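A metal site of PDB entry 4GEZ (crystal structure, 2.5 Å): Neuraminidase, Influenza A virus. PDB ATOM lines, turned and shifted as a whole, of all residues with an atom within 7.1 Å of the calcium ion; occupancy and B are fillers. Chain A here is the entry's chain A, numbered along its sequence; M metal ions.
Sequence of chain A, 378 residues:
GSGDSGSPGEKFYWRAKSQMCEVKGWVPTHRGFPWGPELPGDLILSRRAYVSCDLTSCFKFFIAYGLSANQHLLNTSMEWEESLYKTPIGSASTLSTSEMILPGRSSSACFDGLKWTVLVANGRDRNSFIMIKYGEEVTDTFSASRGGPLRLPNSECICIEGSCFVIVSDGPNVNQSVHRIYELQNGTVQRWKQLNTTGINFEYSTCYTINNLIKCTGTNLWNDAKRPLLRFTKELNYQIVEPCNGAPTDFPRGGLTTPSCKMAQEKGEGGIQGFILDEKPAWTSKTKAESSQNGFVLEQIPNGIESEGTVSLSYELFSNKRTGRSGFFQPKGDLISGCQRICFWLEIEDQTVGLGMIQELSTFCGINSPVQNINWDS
O of Asn 220 is bound to the calcium ion (2.3 Å).
OD2 of Asp 250 binds the calcium ion.
The backbone carbonyl oxygen (O) of Gly 270 is bound to the calcium ion (2.4 Å).
O of Asp 224 is bound to the calcium ion (2.4 Å).
O of Gly 268 is bound to the calcium ion.
The calcium ion has five donor atoms within binding distance.
OD1 of Asn 220 lies within hydrogen-bond range of N of Trp 222.
The side-chain amide oxygen of Asn 223 is in hydrogen-bond range of the side-chain amide nitrogen of Asn 220 (3.1 Å).
The backbone NH (N) of Asp 250 sits close to the backbone carbonyl oxygen (O) of Ala 225 (3.2 Å).
OD1 of Asp 250 lies within hydrogen-bond range of N of Ile 272, at 3.0 Å.
O of Asp 250 lies within hydrogen-bond range of NH1 of Arg 253 (2.9 Å).
The backbone carbonyl oxygen of Leu 221 lies within hydrogen-bond range of the backbone NH of Gly 270 (2.9 Å).
OD1 of Asp 224 sits at hydrogen-bond distance from N of Lys 226, at 2.8 Å.
The backbone NH (N) of Ala 264 lies within hydrogen-bond range of the side-chain carboxylate (OD1) of Asp 224 (3.0 Å).
Gly 271 touches the calcium ion (CA to CA, 3.98 Å).
The nearest printed residue that does not touch the calcium ion is Ala 225 (4.2 Å).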
ATOM      1  N   THR A 219     -18.265 -11.263  37.054  1.00  0.00           N
ATOM      2  CA  THR A 219     -17.960 -11.444  35.644  1.00  0.00           C
ATOM      3  C   THR A 219     -18.767 -12.622  35.153  1.00  0.00           C
ATOM      4  O   THR A 219     -18.694 -13.711  35.725  1.00  0.00           O
ATOM      5  CB  THR A 219     -16.463 -11.745  35.425  1.00  0.00           C
ATOM      6  OG1 THR A 219     -15.662 -10.663  35.933  1.00  0.00           O
ATOM      7  CG2 THR A 219     -16.165 -11.913  33.935  1.00  0.00           C
ATOM      8  N   ASN A 220     -19.540 -12.416  34.087  1.00  0.00           N
ATOM      9  CA  ASN A 220     -20.339 -13.500  33.528  1.00  0.00           C
ATOM     10  C   ASN A 220     -19.614 -14.121  32.342  1.00  0.00           C
ATOM     11  O   ASN A 220     -19.441 -13.491  31.307  1.00  0.00           O
ATOM     12  CB  ASN A 220     -21.719 -12.978  33.107  1.00  0.00           C
ATOM     13  CG  ASN A 220     -22.688 -14.092  32.759  1.00  0.00           C
ATOM     14  OD1 ASN A 220     -22.307 -15.143  32.248  1.00  0.00           O
ATOM     15  ND2 ASN A 220     -23.970 -13.865  33.042  1.00  0.00           N
ATOM     16  N   LEU A 221     -19.173 -15.365  32.522  1.00  0.00           N
ATOM     17  CA  LEU A 221     -18.433 -16.073  31.498  1.00  0.00           C
ATOM     18  C   LEU A 221     -19.363 -16.852  30.576  1.00  0.00           C
ATOM     19  O   LEU A 221     -18.903 -17.508  29.641  1.00  0.00           O
ATOM     20  CB  LEU A 221     -17.427 -17.032  32.139  1.00  0.00           C
ATOM     21  CG  LEU A 221     -16.378 -16.371  33.040  1.00  0.00           C
ATOM     22  CD1 LEU A 221     -15.475 -17.394  33.708  1.00  0.00           C
ATOM     23  CD2 LEU A 221     -15.566 -15.382  32.252  1.00  0.00           C
ATOM     24  N   TRP A 222     -20.659 -16.742  30.820  1.00  0.00           N
ATOM     25  CA  TRP A 222     -21.626 -17.623  30.179  1.00  0.00           C
ATOM     26  C   TRP A 222     -22.412 -16.939  29.053  1.00  0.00           C
ATOM     27  O   TRP A 222     -22.255 -17.276  27.885  1.00  0.00           O
ATOM     28  CB  TRP A 222     -22.593 -18.181  31.230  1.00  0.00           C
ATOM     29  CG  TRP A 222     -23.682 -19.055  30.663  1.00  0.00           C
ATOM     30  CD1 TRP A 222     -23.640 -19.744  29.474  1.00  0.00           C
ATOM     31  CD2 TRP A 222     -24.966 -19.325  31.233  1.00  0.00           C
ATOM     32  NE1 TRP A 222     -24.816 -20.427  29.292  1.00  0.00           N
ATOM     33  CE2 TRP A 222     -25.647 -20.180  30.351  1.00  0.00           C
ATOM     34  CE3 TRP A 222     -25.612 -18.930  32.413  1.00  0.00           C
ATOM     35  CZ2 TRP A 222     -26.943 -20.651  30.603  1.00  0.00           C
ATOM     36  CZ3 TRP A 222     -26.895 -19.391  32.669  1.00  0.00           C
ATOM     37  CH2 TRP A 222     -27.543 -20.250  31.764  1.00  0.00           C
ATOM     38  N   ASN A 223     -23.237 -15.964  29.422  1.00  0.00           N
ATOM     39  CA  ASN A 223     -24.238 -15.416  28.501  1.00  0.00           C
ATOM     40  C   ASN A 223     -24.474 -13.911  28.635  1.00  0.00           C
ATOM     41  O   ASN A 223     -25.546 -13.419  28.304  1.00  0.00           O
ATOM     42  CB  ASN A 223     -25.562 -16.172  28.679  1.00  0.00           C
ATOM     43  CG  ASN A 223     -26.067 -16.124  30.114  1.00  0.00           C
ATOM     44  OD1 ASN A 223     -25.331 -15.716  31.018  1.00  0.00           O
ATOM     45  ND2 ASN A 223     -27.295 -16.554  30.336  1.00  0.00           N
ATOM     46  N   ASP A 224     -23.464 -13.185  29.131  1.00  0.00           N
ATOM     47  CA  ASP A 224     -23.635 -11.758  29.394  1.00  0.00           C
ATOM     48  C   ASP A 224     -22.351 -10.930  29.251  1.00  0.00           C
ATOM     49  O   ASP A 224     -21.291 -11.312  29.761  1.00  0.00           O
ATOM     50  CB  ASP A 224     -24.225 -11.568  30.781  1.00  0.00           C
ATOM     51  CG  ASP A 224     -24.724 -10.156  31.024  1.00  0.00           C
ATOM     52  OD1 ASP A 224     -24.839  -9.380  30.057  1.00  0.00           O
ATOM     53  OD2 ASP A 224     -24.982  -9.838  32.197  1.00  0.00           O
ATOM     54  N   ALA A 225     -22.465  -9.787  28.579  1.00  0.00           N
ATOM     55  CA  ALA A 225     -21.353  -8.863  28.443  1.00  0.00           C
ATOM     56  C   ALA A 225     -21.507  -7.687  29.409  1.00  0.00           C
ATOM     57  O   ALA A 225     -20.623  -6.840  29.494  1.00  0.00           O
ATOM     58  CB  ALA A 225     -21.246  -8.356  27.014  1.00  0.00           C
ATOM     59  N   LYS A 226     -22.638  -7.629  30.106  1.00  0.00           N
ATOM     60  CA  LYS A 226     -22.753  -6.712  31.236  1.00  0.00           C
ATOM     61  C   LYS A 226     -22.248  -7.429  32.478  1.00  0.00           C
ATOM     62  O   LYS A 226     -22.236  -8.668  32.527  1.00  0.00           O
ATOM     63  CB  LYS A 226     -24.200  -6.243  31.452  1.00  0.00           C
ATOM     64  CG  LYS A 226     -24.682  -5.130  30.529  1.00  0.00           C
ATOM     65  CD  LYS A 226     -26.154  -4.820  30.769  1.00  0.00           C
ATOM     66  CE  LYS A 226     -26.598  -3.596  29.992  1.00  0.00           C
ATOM     67  NZ  LYS A 226     -27.995  -3.186  30.337  1.00  0.00           N
ATOM     68  N   ASP A 250     -17.707  -5.775  30.048  1.00  0.00           N
ATOM     69  CA  ASP A 250     -16.952  -7.031  30.037  1.00  0.00           C
ATOM     70  C   ASP A 250     -16.084  -7.098  28.777  1.00  0.00           C
ATOM     71  O   ASP A 250     -16.291  -6.324  27.836  1.00  0.00           O
ATOM     72  CB  ASP A 250     -17.940  -8.198  30.049  1.00  0.00           C
ATOM     73  CG  ASP A 250     -17.309  -9.486  30.521  1.00  0.00           C
ATOM     74  OD1 ASP A 250     -16.069  -9.530  30.689  1.00  0.00           O
ATOM     75  OD2 ASP A 250     -18.073 -10.470  30.704  1.00  0.00           O
ATOM     76  N   PHE A 251     -15.109  -7.998  28.764  1.00  0.00           N
ATOM     77  CA  PHE A 251     -14.379  -8.328  27.546  1.00  0.00           C
ATOM     78  C   PHE A 251     -14.279  -9.843  27.406  1.00  0.00           C
ATOM     79  O   PHE A 251     -13.789 -10.504  28.312  1.00  0.00           O
ATOM     80  CB  PHE A 251     -12.965  -7.714  27.534  1.00  0.00           C
ATOM     81  CG  PHE A 251     -12.302  -7.783  26.183  1.00  0.00           C
ATOM     82  CD1 PHE A 251     -11.626  -8.927  25.775  1.00  0.00           C
ATOM     83  CD2 PHE A 251     -12.348  -6.694  25.324  1.00  0.00           C
ATOM     84  CE1 PHE A 251     -11.022  -9.000  24.537  1.00  0.00           C
ATOM     85  CE2 PHE A 251     -11.736  -6.745  24.084  1.00  0.00           C
ATOM     86  CZ  PHE A 251     -11.076  -7.902  23.686  1.00  0.00           C
ATOM     87  N   PRO A 252     -14.730 -10.391  26.267  1.00  0.00           N
ATOM     88  CA  PRO A 252     -15.218  -9.672  25.087  1.00  0.00           C
ATOM     89  C   PRO A 252     -16.630  -9.126  25.287  1.00  0.00           C
ATOM     90  O   PRO A 252     -17.293  -9.464  26.276  1.00  0.00           O
ATOM     91  CB  PRO A 252     -15.228 -10.752  24.012  1.00  0.00           C
ATOM     92  CG  PRO A 252     -15.454 -12.019  24.757  1.00  0.00           C
ATOM     93  CD  PRO A 252     -14.759 -11.847  26.077  1.00  0.00           C
ATOM     94  N   ARG A 253     -17.078  -8.302  24.346  1.00  0.00           N
ATOM     95  CA  ARG A 253     -18.410  -7.712  24.387  1.00  0.00           C
ATOM     96  C   ARG A 253     -18.776  -7.183  23.004  1.00  0.00           C
ATOM     97  O   ARG A 253     -17.901  -7.003  22.157  1.00  0.00           O
ATOM     98  CB  ARG A 253     -18.469  -6.566  25.395  1.00  0.00           C
ATOM     99  CG  ARG A 253     -17.640  -5.363  24.972  1.00  0.00           C
ATOM    100  CD  ARG A 253     -17.898  -4.137  25.833  1.00  0.00           C
ATOM    101  NE  ARG A 253     -17.013  -3.033  25.482  1.00  0.00           N
ATOM    102  CZ  ARG A 253     -15.766  -2.910  25.932  1.00  0.00           C
ATOM    103  NH1 ARG A 253     -15.257  -3.827  26.735  1.00  0.00           N
ATOM    104  NH2 ARG A 253     -15.026  -1.876  25.563  1.00  0.00           N
ATOM    105  N   ALA A 264     -26.710  -8.302  28.037  1.00  0.00           N
ATOM    106  CA  ALA A 264     -26.180  -8.089  26.699  1.00  0.00           C
ATOM    107  C   ALA A 264     -25.611  -9.399  26.189  1.00  0.00           C
ATOM    108  O   ALA A 264     -24.499  -9.780  26.541  1.00  0.00           O
ATOM    109  CB  ALA A 264     -25.100  -7.022  26.723  1.00  0.00           C
ATOM    110  N   LYS A 267     -21.755 -11.752  22.251  1.00  0.00           N
ATOM    111  CA  LYS A 267     -20.413 -12.028  22.761  1.00  0.00           C
ATOM    112  C   LYS A 267     -20.393 -12.133  24.282  1.00  0.00           C
ATOM    113  O   LYS A 267     -19.468 -11.646  24.944  1.00  0.00           O
ATOM    114  CB  LYS A 267     -19.457 -10.936  22.276  1.00  0.00           C
ATOM    115  CG  LYS A 267     -19.295 -10.909  20.768  1.00  0.00           C
ATOM    116  CD  LYS A 267     -18.144 -10.012  20.334  1.00  0.00           C
ATOM    117  CE  LYS A 267     -18.391  -9.469  18.933  1.00  0.00           C
ATOM    118  NZ  LYS A 267     -17.637  -8.206  18.653  1.00  0.00           N
ATOM    119  N   GLY A 268     -21.416 -12.775  24.839  1.00  0.00           N
ATOM    120  CA  GLY A 268     -21.548 -12.959  26.272  1.00  0.00           C
ATOM    121  C   GLY A 268     -20.602 -14.027  26.808  1.00  0.00           C
ATOM    122  O   GLY A 268     -20.173 -13.964  27.970  1.00  0.00           O
ATOM    123  N   GLU A 269     -20.304 -15.009  25.972  1.00  0.00           N
ATOM    124  CA  GLU A 269     -19.342 -16.063  26.316  1.00  0.00           C
ATOM    125  C   GLU A 269     -17.972 -15.495  26.608  1.00  0.00           C
ATOM    126  O   GLU A 269     -17.484 -14.617  25.884  1.00  0.00           O
ATOM    127  CB  GLU A 269     -19.230 -17.105  25.198  1.00  0.00           C
ATOM    128  CG  GLU A 269     -19.743 -18.486  25.567  1.00  0.00           C
ATOM    129  CD  GLU A 269     -19.109 -19.583  24.743  1.00  0.00           C
ATOM    130  OE1 GLU A 269     -19.847 -20.263  23.993  1.00  0.00           O
ATOM    131  OE2 GLU A 269     -17.883 -19.789  24.842  1.00  0.00           O
ATOM    132  N   GLY A 270     -17.354 -15.962  27.692  1.00  0.00           N
ATOM    133  CA  GLY A 270     -16.055 -15.454  28.062  1.00  0.00           C
ATOM    134  C   GLY A 270     -16.225 -14.247  28.958  1.00  0.00           C
ATOM    135  O   GLY A 270     -17.350 -13.899  29.329  1.00  0.00           O
ATOM    136  N   GLY A 271     -15.116 -13.621  29.315  1.00  0.00           N
ATOM    137  CA  GLY A 271     -15.160 -12.457  30.168  1.00  0.00           C
ATOM    138  C   GLY A 271     -13.806 -12.235  30.810  1.00  0.00           C
ATOM    139  O   GLY A 271     -12.900 -13.045  30.648  1.00  0.00           O
ATOM    140  N   ILE A 272     -13.679 -11.148  31.549  1.00  0.00           N
ATOM    141  CA  ILE A 272     -12.456 -10.885  32.299  1.00  0.00           C
ATOM    142  C   ILE A 272     -12.834 -10.178  33.574  1.00  0.00           C
ATOM    143  O   ILE A 272     -13.826  -9.466  33.614  1.00  0.00           O
ATOM    144  CB  ILE A 272     -11.441 -10.046  31.477  1.00  0.00           C
ATOM    145  CG1 ILE A 272     -10.101  -9.980  32.197  1.00  0.00           C
ATOM    146  CG2 ILE A 272     -11.985  -8.645  31.226  1.00  0.00           C
ATOM    147  CD1 ILE A 272      -8.930  -9.724  31.289  1.00  0.00           C
HETATM  148 CA    CA M   1     -19.068 -12.228  29.462  1.00  0.00          CA
